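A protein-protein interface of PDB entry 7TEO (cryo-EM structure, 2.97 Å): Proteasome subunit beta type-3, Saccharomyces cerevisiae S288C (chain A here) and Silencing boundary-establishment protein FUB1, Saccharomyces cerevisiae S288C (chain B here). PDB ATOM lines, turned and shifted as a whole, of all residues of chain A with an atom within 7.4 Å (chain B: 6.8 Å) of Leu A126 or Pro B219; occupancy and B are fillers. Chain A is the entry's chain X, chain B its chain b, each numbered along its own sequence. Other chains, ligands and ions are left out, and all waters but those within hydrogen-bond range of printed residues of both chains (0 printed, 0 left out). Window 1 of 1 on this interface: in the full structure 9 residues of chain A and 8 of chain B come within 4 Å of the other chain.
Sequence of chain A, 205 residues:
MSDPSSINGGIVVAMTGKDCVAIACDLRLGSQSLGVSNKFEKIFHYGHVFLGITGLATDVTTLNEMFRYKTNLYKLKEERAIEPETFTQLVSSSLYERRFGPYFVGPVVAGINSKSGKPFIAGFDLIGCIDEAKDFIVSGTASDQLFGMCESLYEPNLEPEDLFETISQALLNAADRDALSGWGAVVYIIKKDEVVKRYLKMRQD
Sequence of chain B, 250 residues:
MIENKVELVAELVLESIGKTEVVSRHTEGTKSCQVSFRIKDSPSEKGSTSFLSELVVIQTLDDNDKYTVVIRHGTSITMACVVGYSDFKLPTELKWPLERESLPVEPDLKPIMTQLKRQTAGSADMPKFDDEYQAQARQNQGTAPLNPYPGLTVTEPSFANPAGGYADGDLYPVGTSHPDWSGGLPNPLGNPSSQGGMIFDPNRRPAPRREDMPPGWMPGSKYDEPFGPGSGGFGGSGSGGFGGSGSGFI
The side-chain amino group (NZ) of Lys B222 is in hydrogen-bond range of the side-chain sulfur (SG) of Cys A129.
O of Tyr B149 lies within hydrogen-bond range of ND2 of Asn B147 (2.7 Å). The side-chain carboxylate (OD1) of Asp A125 lies within hydrogen-bond range of the backbone NH (N) of Ile A127, 3.1 Å away. The backbone carbonyl oxygen of Met B218 is in hydrogen-bond range of the side-chain hydroxyl of Ser B221. The side-chain carboxylate (OD1) of Asp A125 is in hydrogen-bond range of the backbone NH (N) of Gly A128 (2.8 Å). The side-chain carboxylate (OD1) of Asp A125 sits at hydrogen-bond distance from the backbone NH (N) of Cys A129 (2.7 Å). OD1 of Asp A3 lies within hydrogen-bond range of N of Ser A5.
Among the printed residues, merely in contact across the chains: Asp A3 with Tyr B149 (3.4 Å), Pro A4 with Tyr B149 (3.4 Å), Arg A99 with Met B218 (3.2 Å), Pro A102 with Met B218 (3.8 Å), Phe A104 with Tyr B149 (3.6 Å), Phe A104 with Pro B150 (3.5 Å), Asp A125 with Lys B222 (3.5 Å) and Leu A126 with Pro B219 (3.0 Å).
Of the printed residues of chain B, Asp A3 touches Tyr B149 (3.4 Å). Of the printed residues of chain B, Pro A4 touches Tyr B149. Of the printed residues of chain B, Arg A99 touches Met B218 (3.2 Å). Of the printed residues of chain B, Pro A102 touches Met B218. Of chain B, only Pro B219 comes within 4 Å of Leu A126. Of chain A, only Leu A126 comes within 4 Å of Pro B219. The nearest residue of chain B that does not touch Leu A126 is Gly B220 (4.1 Å). The nearest residue of chain A that does not touch Pro B219 is Phe A104 (4.5 Å).
Of the 23 printed residues of chain A, 8 touch a printed residue of chain B. Along chain A the printed residues that touch a printed residue of chain B span positions 3 to 129. Of the 12 printed residues of chain B, 5 touch a printed residue of chain A. Hydrophobic or aromatic side chains of chain B within 4 Å of the printed part of chain A: Tyr B149 and Met B218. Among the printed residues, no Asp or Glu carboxylate lies within 4 Å of a Lys or Arg side-chain nitrogen of the other chain.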
ATOM      1  N   ASP A   3     -15.603  14.223  -8.350  1.00  0.00           N
ATOM      2  CA  ASP A   3     -15.260  13.392  -7.162  1.00  0.00           C
ATOM      3  C   ASP A   3     -16.163  13.788  -5.992  1.00  0.00           C
ATOM      4  O   ASP A   3     -16.182  14.953  -5.597  1.00  0.00           O
ATOM      5  CB  ASP A   3     -13.782  13.569  -6.797  1.00  0.00           C
ATOM      6  CG  ASP A   3     -13.359  12.713  -5.616  1.00  0.00           C
ATOM      7  OD1 ASP A   3     -14.233  12.195  -4.892  1.00  0.00           O
ATOM      8  OD2 ASP A   3     -12.137  12.561  -5.411  1.00  0.00           O
ATOM      9  N   PRO A   4     -16.917  12.832  -5.439  1.00  0.00           N
ATOM     10  CA  PRO A   4     -17.835  13.183  -4.343  1.00  0.00           C
ATOM     11  C   PRO A   4     -17.156  13.832  -3.152  1.00  0.00           C
ATOM     12  O   PRO A   4     -17.758  14.704  -2.513  1.00  0.00           O
ATOM     13  CB  PRO A   4     -18.456  11.831  -3.971  1.00  0.00           C
ATOM     14  CG  PRO A   4     -18.401  11.049  -5.224  1.00  0.00           C
ATOM     15  CD  PRO A   4     -17.103  11.435  -5.868  1.00  0.00           C
ATOM     16  N   SER A   5     -15.924  13.442  -2.828  1.00  0.00           N
ATOM     17  CA  SER A   5     -15.245  14.038  -1.685  1.00  0.00           C
ATOM     18  C   SER A   5     -14.727  15.436  -1.994  1.00  0.00           C
ATOM     19  O   SER A   5     -14.617  16.268  -1.086  1.00  0.00           O
ATOM     20  CB  SER A   5     -14.091  13.141  -1.236  1.00  0.00           C
ATOM     21  OG  SER A   5     -14.564  11.870  -0.829  1.00  0.00           O
ATOM     22  N   THR A  54     -16.167  16.096   6.770  1.00  0.00           N
ATOM     23  CA  THR A  54     -15.946  16.650   5.446  1.00  0.00           C
ATOM     24  C   THR A  54     -16.441  15.668   4.390  1.00  0.00           C
ATOM     25  O   THR A  54     -16.794  14.525   4.683  1.00  0.00           O
ATOM     26  CB  THR A  54     -14.468  16.957   5.222  1.00  0.00           C
ATOM     27  OG1 THR A  54     -13.700  15.760   5.394  1.00  0.00           O
ATOM     28  CG2 THR A  54     -13.993  17.996   6.204  1.00  0.00           C
ATOM     29  N   GLY A  55     -16.460  16.128   3.144  1.00  0.00           N
ATOM     30  CA  GLY A  55     -16.853  15.278   2.041  1.00  0.00           C
ATOM     31  C   GLY A  55     -18.160  15.711   1.415  1.00  0.00           C
ATOM     32  O   GLY A  55     -18.555  16.874   1.525  1.00  0.00           O
ATOM     33  N   LEU A  63     -25.377  11.773   7.816  1.00  0.00           N
ATOM     34  CA  LEU A  63     -24.708  11.227   8.987  1.00  0.00           C
ATOM     35  C   LEU A  63     -24.992  12.060  10.226  1.00  0.00           C
ATOM     36  O   LEU A  63     -25.077  11.517  11.330  1.00  0.00           O
ATOM     37  CB  LEU A  63     -23.205  11.128   8.739  1.00  0.00           C
ATOM     38  CG  LEU A  63     -22.755  10.218   7.597  1.00  0.00           C
ATOM     39  CD1 LEU A  63     -21.325   9.803   7.829  1.00  0.00           C
ATOM     40  CD2 LEU A  63     -23.642   9.001   7.456  1.00  0.00           C
ATOM     41  N   SER A  94     -20.989   2.173  11.957  1.00  0.00           N
ATOM     42  CA  SER A  94     -22.001   2.693  11.045  1.00  0.00           C
ATOM     43  C   SER A  94     -21.427   2.958   9.660  1.00  0.00           C
ATOM     44  O   SER A  94     -22.121   2.764   8.657  1.00  0.00           O
ATOM     45  CB  SER A  94     -22.610   3.972  11.614  1.00  0.00           C
ATOM     46  OG  SER A  94     -23.193   3.735  12.881  1.00  0.00           O
ATOM     47  N   LEU A  95     -20.174   3.406   9.584  1.00  0.00           N
ATOM     48  CA  LEU A  95     -19.568   3.670   8.284  1.00  0.00           C
ATOM     49  C   LEU A  95     -19.332   2.380   7.511  1.00  0.00           C
ATOM     50  O   LEU A  95     -19.555   2.328   6.297  1.00  0.00           O
ATOM     51  CB  LEU A  95     -18.256   4.429   8.461  1.00  0.00           C
ATOM     52  CG  LEU A  95     -18.394   5.915   8.782  1.00  0.00           C
ATOM     53  CD1 LEU A  95     -17.115   6.440   9.401  1.00  0.00           C
ATOM     54  CD2 LEU A  95     -18.742   6.692   7.529  1.00  0.00           C
ATOM     55  N   TYR A  96     -18.873   1.329   8.193  1.00  0.00           N
ATOM     56  CA  TYR A  96     -18.604   0.074   7.502  1.00  0.00           C
ATOM     57  C   TYR A  96     -19.888  -0.637   7.100  1.00  0.00           C
ATOM     58  O   TYR A  96     -19.862  -1.499   6.215  1.00  0.00           O
ATOM     59  CB  TYR A  96     -17.752  -0.847   8.373  1.00  0.00           C
ATOM     60  CG  TYR A  96     -17.193  -2.023   7.606  1.00  0.00           C
ATOM     61  CD1 TYR A  96     -16.063  -1.883   6.811  1.00  0.00           C
ATOM     62  CD2 TYR A  96     -17.801  -3.267   7.666  1.00  0.00           C
ATOM     63  CE1 TYR A  96     -15.554  -2.951   6.103  1.00  0.00           C
ATOM     64  CE2 TYR A  96     -17.298  -4.340   6.960  1.00  0.00           C
ATOM     65  CZ  TYR A  96     -16.175  -4.177   6.181  1.00  0.00           C
ATOM     66  OH  TYR A  96     -15.671  -5.244   5.478  1.00  0.00           O
ATOM     67  N   ARG A  98     -22.188   0.236   5.281  1.00  0.00           N
ATOM     68  CA  ARG A  98     -22.383   0.437   3.855  1.00  0.00           C
ATOM     69  C   ARG A  98     -21.105   0.207   3.060  1.00  0.00           C
ATOM     70  O   ARG A  98     -20.845   0.932   2.094  1.00  0.00           O
ATOM     71  CB  ARG A  98     -22.908   1.845   3.596  1.00  0.00           C
ATOM     72  CG  ARG A  98     -24.301   2.084   4.135  1.00  0.00           C
ATOM     73  CD  ARG A  98     -24.738   3.476   3.791  1.00  0.00           C
ATOM     74  NE  ARG A  98     -26.031   3.831   4.354  1.00  0.00           N
ATOM     75  CZ  ARG A  98     -27.203   3.622   3.766  1.00  0.00           C
ATOM     76  NH1 ARG A  98     -27.291   3.043   2.576  1.00  0.00           N
ATOM     77  NH2 ARG A  98     -28.317   4.003   4.388  1.00  0.00           N
ATOM     78  N   ARG A  99     -20.304  -0.782   3.452  1.00  0.00           N
ATOM     79  CA  ARG A  99     -18.999  -1.033   2.850  1.00  0.00           C
ATOM     80  C   ARG A  99     -19.008  -0.882   1.334  1.00  0.00           C
ATOM     81  O   ARG A  99     -18.077  -0.312   0.760  1.00  0.00           O
ATOM     82  CB  ARG A  99     -18.517  -2.436   3.223  1.00  0.00           C
ATOM     83  CG  ARG A  99     -17.304  -2.937   2.432  1.00  0.00           C
ATOM     84  CD  ARG A  99     -16.107  -1.998   2.515  1.00  0.00           C
ATOM     85  NE  ARG A  99     -14.925  -2.558   1.870  1.00  0.00           N
ATOM     86  CZ  ARG A  99     -14.628  -2.423   0.584  1.00  0.00           C
ATOM     87  NH1 ARG A  99     -15.412  -1.752  -0.243  1.00  0.00           N
ATOM     88  NH2 ARG A  99     -13.513  -2.976   0.114  1.00  0.00           N
ATOM     89  N   PRO A 102     -20.676   3.125   0.235  1.00  0.00           N
ATOM     90  CA  PRO A 102     -20.278   3.982   1.354  1.00  0.00           C
ATOM     91  C   PRO A 102     -20.624   5.451   1.161  1.00  0.00           C
ATOM     92  O   PRO A 102     -20.714   5.966   0.047  1.00  0.00           O
ATOM     93  CB  PRO A 102     -18.762   3.792   1.392  1.00  0.00           C
ATOM     94  CG  PRO A 102     -18.408   3.640  -0.043  1.00  0.00           C
ATOM     95  CD  PRO A 102     -19.523   2.795  -0.621  1.00  0.00           C
ATOM     96  N   TYR A 103     -20.825   6.118   2.297  1.00  0.00           N
ATOM     97  CA  TYR A 103     -20.823   7.573   2.337  1.00  0.00           C
ATOM     98  C   TYR A 103     -19.449   8.103   1.951  1.00  0.00           C
ATOM     99  O   TYR A 103     -18.423   7.561   2.374  1.00  0.00           O
ATOM    100  CB  TYR A 103     -21.194   8.070   3.732  1.00  0.00           C
ATOM    101  CG  TYR A 103     -22.479   7.522   4.293  1.00  0.00           C
ATOM    102  CD1 TYR A 103     -23.697   8.070   3.935  1.00  0.00           C
ATOM    103  CD2 TYR A 103     -22.466   6.474   5.195  1.00  0.00           C
ATOM    104  CE1 TYR A 103     -24.870   7.583   4.448  1.00  0.00           C
ATOM    105  CE2 TYR A 103     -23.632   5.983   5.729  1.00  0.00           C
ATOM    106  CZ  TYR A 103     -24.834   6.536   5.343  1.00  0.00           C
ATOM    107  OH  TYR A 103     -26.008   6.055   5.862  1.00  0.00           O
ATOM    108  N   PHE A 104     -19.432   9.165   1.152  1.00  0.00           N
ATOM    109  CA  PHE A 104     -18.184   9.783   0.708  1.00  0.00           C
ATOM    110  C   PHE A 104     -17.834  10.938   1.646  1.00  0.00           C
ATOM    111  O   PHE A 104     -17.920  12.118   1.306  1.00  0.00           O
ATOM    112  CB  PHE A 104     -18.316  10.243  -0.734  1.00  0.00           C
ATOM    113  CG  PHE A 104     -18.365   9.116  -1.716  1.00  0.00           C
ATOM    114  CD1 PHE A 104     -17.212   8.451  -2.080  1.00  0.00           C
ATOM    115  CD2 PHE A 104     -19.567   8.715  -2.268  1.00  0.00           C
ATOM    116  CE1 PHE A 104     -17.254   7.409  -2.981  1.00  0.00           C
ATOM    117  CE2 PHE A 104     -19.614   7.675  -3.169  1.00  0.00           C
ATOM    118  CZ  PHE A 104     -18.458   7.020  -3.524  1.00  0.00           C
ATOM    119  N   VAL A 105     -17.430  10.565   2.860  1.00  0.00           N
ATOM    120  CA  VAL A 105     -17.154  11.521   3.921  1.00  0.00           C
ATOM    121  C   VAL A 105     -15.862  11.135   4.623  1.00  0.00           C
ATOM    122  O   VAL A 105     -15.439   9.978   4.609  1.00  0.00           O
ATOM    123  CB  VAL A 105     -18.299  11.588   4.952  1.00  0.00           C
ATOM    124  CG1 VAL A 105     -19.560  12.138   4.318  1.00  0.00           C
ATOM    125  CG2 VAL A 105     -18.551  10.212   5.545  1.00  0.00           C
ATOM    126  N   GLY A 106     -15.236  12.128   5.245  1.00  0.00           N
ATOM    127  CA  GLY A 106     -14.220  11.875   6.235  1.00  0.00           C
ATOM    128  C   GLY A 106     -14.603  12.520   7.550  1.00  0.00           C
ATOM    129  O   GLY A 106     -14.531  13.742   7.708  1.00  0.00           O
ATOM    130  N   PRO A 107     -15.014  11.714   8.522  1.00  0.00           N
ATOM    131  CA  PRO A 107     -15.335  12.259   9.845  1.00  0.00           C
ATOM    132  C   PRO A 107     -14.103  12.435  10.722  1.00  0.00           C
ATOM    133  O   PRO A 107     -13.028  11.893  10.463  1.00  0.00           O
ATOM    134  CB  PRO A 107     -16.287  11.213  10.440  1.00  0.00           C
ATOM    135  CG  PRO A 107     -16.802  10.457   9.274  1.00  0.00           C
ATOM    136  CD  PRO A 107     -15.668  10.414   8.309  1.00  0.00           C
ATOM    137  N   PHE A 124     -11.222   9.109  10.342  1.00  0.00           N
ATOM    138  CA  PHE A 124     -11.798   7.995   9.604  1.00  0.00           C
ATOM    139  C   PHE A 124     -11.557   8.181   8.113  1.00  0.00           C
ATOM    140  O   PHE A 124     -11.266   9.280   7.638  1.00  0.00           O
ATOM    141  CB  PHE A 124     -13.299   7.879   9.867  1.00  0.00           C
ATOM    142  CG  PHE A 124     -13.640   7.499  11.268  1.00  0.00           C
ATOM    143  CD1 PHE A 124     -13.576   6.183  11.674  1.00  0.00           C
ATOM    144  CD2 PHE A 124     -14.036   8.461  12.177  1.00  0.00           C
ATOM    145  CE1 PHE A 124     -13.891   5.833  12.963  1.00  0.00           C
ATOM    146  CE2 PHE A 124     -14.355   8.117  13.466  1.00  0.00           C
ATOM    147  CZ  PHE A 124     -14.284   6.802  13.859  1.00  0.00           C
ATOM    148  N   ASP A 125     -11.681   7.078   7.381  1.00  0.00           N
ATOM    149  CA  ASP A 125     -11.779   7.088   5.932  1.00  0.00           C
ATOM    150  C   ASP A 125     -13.240   6.881   5.526  1.00  0.00           C
ATOM    151  O   ASP A 125     -14.149   6.891   6.356  1.00  0.00           O
ATOM    152  CB  ASP A 125     -10.861   6.027   5.319  1.00  0.00           C
ATOM    153  CG  ASP A 125     -11.318   4.613   5.612  1.00  0.00           C
ATOM    154  OD1 ASP A 125     -12.282   4.442   6.384  1.00  0.00           O
ATOM    155  OD2 ASP A 125     -10.709   3.668   5.068  1.00  0.00           O
ATOM    156  N   LEU A 126     -13.464   6.698   4.223  1.00  0.00           N
ATOM    157  CA  LEU A 126     -14.824   6.529   3.717  1.00  0.00           C
ATOM    158  C   LEU A 126     -15.568   5.410   4.430  1.00  0.00           C
ATOM    159  O   LEU A 126     -16.766   5.538   4.704  1.00  0.00           O
ATOM    160  CB  LEU A 126     -14.796   6.229   2.219  1.00  0.00           C
ATOM    161  CG  LEU A 126     -14.934   7.398   1.251  1.00  0.00           C
ATOM    162  CD1 LEU A 126     -14.006   8.547   1.615  1.00  0.00           C
ATOM    163  CD2 LEU A 126     -14.658   6.908  -0.158  1.00  0.00           C
ATOM    164  N   ILE A 127     -14.883   4.310   4.731  1.00  0.00           N
ATOM    165  CA  ILE A 127     -15.513   3.084   5.198  1.00  0.00           C
ATOM    166  C   ILE A 127     -15.031   2.683   6.592  1.00  0.00           C
ATOM    167  O   ILE A 127     -14.925   1.503   6.895  1.00  0.00           O
ATOM    168  CB  ILE A 127     -15.316   1.948   4.175  1.00  0.00           C
ATOM    169  CG1 ILE A 127     -13.830   1.644   3.982  1.00  0.00           C
ATOM    170  CG2 ILE A 127     -15.972   2.303   2.863  1.00  0.00           C
ATOM    171  CD1 ILE A 127     -13.565   0.389   3.170  1.00  0.00           C
ATOM    172  N   GLY A 128     -14.738   3.660   7.446  1.00  0.00           N
ATOM    173  CA  GLY A 128     -14.648   3.397   8.869  1.00  0.00           C
ATOM    174  C   GLY A 128     -13.326   2.885   9.388  1.00  0.00           C
ATOM    175  O   GLY A 128     -13.303   2.206  10.420  1.00  0.00           O
ATOM    176  N   CYS A 129     -12.217   3.182   8.716  1.00  0.00           N
ATOM    177  CA  CYS A 129     -10.916   2.812   9.259  1.00  0.00           C
ATOM    178  C   CYS A 129     -10.561   3.765  10.393  1.00  0.00           C
ATOM    179  O   CYS A 129     -10.335   4.955  10.156  1.00  0.00           O
ATOM    180  CB  CYS A 129      -9.841   2.845   8.170  1.00  0.00           C
ATOM    181  SG  CYS A 129      -8.150   2.729   8.789  1.00  0.00           S
ATOM    182  N   ASN B 147     -18.493   2.104 -12.450  1.00  0.00           N
ATOM    183  CA  ASN B 147     -18.861   3.366 -11.832  1.00  0.00           C
ATOM    184  C   ASN B 147     -17.637   3.946 -11.133  1.00  0.00           C
ATOM    185  O   ASN B 147     -17.051   3.278 -10.270  1.00  0.00           O
ATOM    186  CB  ASN B 147     -19.995   3.155 -10.829  1.00  0.00           C
ATOM    187  CG  ASN B 147     -20.588   4.457 -10.333  1.00  0.00           C
ATOM    188  OD1 ASN B 147     -20.479   5.492 -10.987  1.00  0.00           O
ATOM    189  ND2 ASN B 147     -21.224   4.410  -9.168  1.00  0.00           N
ATOM    190  N   PRO B 148     -17.214   5.169 -11.465  1.00  0.00           N
ATOM    191  CA  PRO B 148     -16.013   5.709 -10.810  1.00  0.00           C
ATOM    192  C   PRO B 148     -16.132   5.744  -9.302  1.00  0.00           C
ATOM    193  O   PRO B 148     -15.121   5.608  -8.601  1.00  0.00           O
ATOM    194  CB  PRO B 148     -15.898   7.121 -11.402  1.00  0.00           C
ATOM    195  CG  PRO B 148     -16.611   7.043 -12.699  1.00  0.00           C
ATOM    196  CD  PRO B 148     -17.755   6.108 -12.462  1.00  0.00           C
ATOM    197  N   TYR B 149     -17.344   5.914  -8.782  1.00  0.00           N
ATOM    198  CA  TYR B 149     -17.586   6.087  -7.353  1.00  0.00           C
ATOM    199  C   TYR B 149     -18.728   5.156  -6.970  1.00  0.00           C
ATOM    200  O   TYR B 149     -19.906   5.520  -7.091  1.00  0.00           O
ATOM    201  CB  TYR B 149     -17.890   7.548  -7.043  1.00  0.00           C
ATOM    202  CG  TYR B 149     -16.794   8.456  -7.546  1.00  0.00           C
ATOM    203  CD1 TYR B 149     -15.526   8.421  -6.982  1.00  0.00           C
ATOM    204  CD2 TYR B 149     -17.013   9.314  -8.613  1.00  0.00           C
ATOM    205  CE1 TYR B 149     -14.515   9.234  -7.450  1.00  0.00           C
ATOM    206  CE2 TYR B 149     -16.007  10.131  -9.088  1.00  0.00           C
ATOM    207  CZ  TYR B 149     -14.758  10.085  -8.504  1.00  0.00           C
ATOM    208  OH  TYR B 149     -13.751  10.898  -8.973  1.00  0.00           O
ATOM    209  N   PRO B 150     -18.421   3.942  -6.510  1.00  0.00           N
ATOM    210  CA  PRO B 150     -19.478   2.941  -6.318  1.00  0.00           C
ATOM    211  C   PRO B 150     -20.516   3.388  -5.301  1.00  0.00           C
ATOM    212  O   PRO B 150     -20.220   4.109  -4.346  1.00  0.00           O
ATOM    213  CB  PRO B 150     -18.713   1.705  -5.833  1.00  0.00           C
ATOM    214  CG  PRO B 150     -17.462   2.247  -5.242  1.00  0.00           C
ATOM    215  CD  PRO B 150     -17.106   3.427  -6.089  1.00  0.00           C
ATOM    216  N   PRO B 208      -6.632   7.068  -9.259  1.00  0.00           N
ATOM    217  CA  PRO B 208      -6.575   5.746  -9.893  1.00  0.00           C
ATOM    218  C   PRO B 208      -7.876   5.416 -10.610  1.00  0.00           C
ATOM    219  O   PRO B 208      -8.932   6.006 -10.370  1.00  0.00           O
ATOM    220  CB  PRO B 208      -6.322   4.788  -8.724  1.00  0.00           C
ATOM    221  CG  PRO B 208      -5.854   5.656  -7.598  1.00  0.00           C
ATOM    222  CD  PRO B 208      -6.542   6.966  -7.793  1.00  0.00           C
ATOM    223  N   ARG B 210     -10.720   2.667 -11.278  1.00  0.00           N
ATOM    224  CA  ARG B 210     -11.273   1.527 -10.556  1.00  0.00           C
ATOM    225  C   ARG B 210     -11.198   0.251 -11.388  1.00  0.00           C
ATOM    226  O   ARG B 210     -11.314  -0.854 -10.845  1.00  0.00           O
ATOM    227  CB  ARG B 210     -12.717   1.825 -10.140  1.00  0.00           C
ATOM    228  CG  ARG B 210     -13.374   0.737  -9.303  1.00  0.00           C
ATOM    229  CD  ARG B 210     -14.781   1.135  -8.884  1.00  0.00           C
ATOM    230  NE  ARG B 210     -15.412   0.123  -8.042  1.00  0.00           N
ATOM    231  CZ  ARG B 210     -16.134  -0.894  -8.493  1.00  0.00           C
ATOM    232  NH1 ARG B 210     -16.338  -1.082  -9.786  1.00  0.00           N
ATOM    233  NH2 ARG B 210     -16.662  -1.750  -7.622  1.00  0.00           N
ATOM    234  N   TRP B 217     -10.294  -2.715  -3.509  1.00  0.00           N
ATOM    235  CA  TRP B 217      -9.999  -1.294  -3.388  1.00  0.00           C
ATOM    236  C   TRP B 217     -11.273  -0.465  -3.494  1.00  0.00           C
ATOM    237  O   TRP B 217     -12.062  -0.632  -4.431  1.00  0.00           O
ATOM    238  CB  TRP B 217      -9.003  -0.870  -4.465  1.00  0.00           C
ATOM    239  CG  TRP B 217      -8.553   0.550  -4.336  1.00  0.00           C
ATOM    240  CD1 TRP B 217      -7.773   1.075  -3.348  1.00  0.00           C
ATOM    241  CD2 TRP B 217      -8.851   1.630  -5.229  1.00  0.00           C
ATOM    242  NE1 TRP B 217      -7.569   2.416  -3.568  1.00  0.00           N
ATOM    243  CE2 TRP B 217      -8.219   2.780  -4.717  1.00  0.00           C
ATOM    244  CE3 TRP B 217      -9.590   1.736  -6.410  1.00  0.00           C
ATOM    245  CZ2 TRP B 217      -8.305   4.019  -5.345  1.00  0.00           C
ATOM    246  CZ3 TRP B 217      -9.673   2.966  -7.032  1.00  0.00           C
ATOM    247  CH2 TRP B 217      -9.035   4.091  -6.498  1.00  0.00           C
ATOM    248  N   MET B 218     -11.470   0.431  -2.528  1.00  0.00           N
ATOM    249  CA  MET B 218     -12.558   1.394  -2.537  1.00  0.00           C
ATOM    250  C   MET B 218     -12.000   2.774  -2.845  1.00  0.00           C
ATOM    251  O   MET B 218     -11.133   3.253  -2.101  1.00  0.00           O
ATOM    252  CB  MET B 218     -13.272   1.409  -1.179  1.00  0.00           C
ATOM    253  CG  MET B 218     -14.348   2.476  -1.033  1.00  0.00           C
ATOM    254  SD  MET B 218     -15.631   2.375  -2.295  1.00  0.00           S
ATOM    255  CE  MET B 218     -16.386   0.802  -1.897  1.00  0.00           C
ATOM    256  N   PRO B 219     -12.436   3.439  -3.917  1.00  0.00           N
ATOM    257  CA  PRO B 219     -11.856   4.746  -4.256  1.00  0.00           C
ATOM    258  C   PRO B 219     -11.900   5.709  -3.081  1.00  0.00           C
ATOM    259  O   PRO B 219     -12.962   5.989  -2.520  1.00  0.00           O
ATOM    260  CB  PRO B 219     -12.732   5.223  -5.419  1.00  0.00           C
ATOM    261  CG  PRO B 219     -13.185   3.970  -6.066  1.00  0.00           C
ATOM    262  CD  PRO B 219     -13.394   2.990  -4.944  1.00  0.00           C
ATOM    263  N   GLY B 220     -10.728   6.222  -2.711  1.00  0.00           N
ATOM    264  CA  GLY B 220     -10.598   7.141  -1.601  1.00  0.00           C
ATOM    265  C   GLY B 220     -10.390   6.493  -0.249  1.00  0.00           C
ATOM    266  O   GLY B 220     -10.256   7.213   0.747  1.00  0.00           O
ATOM    267  N   SER B 221     -10.363   5.165  -0.179  1.00  0.00           N
ATOM    268  CA  SER B 221     -10.132   4.474   1.078  1.00  0.00           C
ATOM    269  C   SER B 221      -8.641   4.237   1.295  1.00  0.00           C
ATOM    270  O   SER B 221      -7.836   4.264   0.360  1.00  0.00           O
ATOM    271  CB  SER B 221     -10.877   3.140   1.100  1.00  0.00           C
ATOM    272  OG  SER B 221     -10.345   2.247   0.137  1.00  0.00           O
ATOM    273  N   LYS B 222      -8.276   3.996   2.552  1.00  0.00           N
ATOM    274  CA  LYS B 222      -6.894   3.687   2.889  1.00  0.00           C
ATOM    275  C   LYS B 222      -6.572   2.265   2.450  1.00  0.00           C
ATOM    276  O   LYS B 222      -7.243   1.313   2.859  1.00  0.00           O
ATOM    277  CB  LYS B 222      -6.656   3.846   4.391  1.00  0.00           C
ATOM    278  CG  LYS B 222      -5.185   3.906   4.771  1.00  0.00           C
ATOM    279  CD  LYS B 222      -4.937   3.415   6.188  1.00  0.00           C
ATOM    280  CE  LYS B 222      -5.622   4.292   7.222  1.00  0.00           C
ATOM    281  NZ  LYS B 222      -5.441   3.766   8.604  1.00  0.00           N
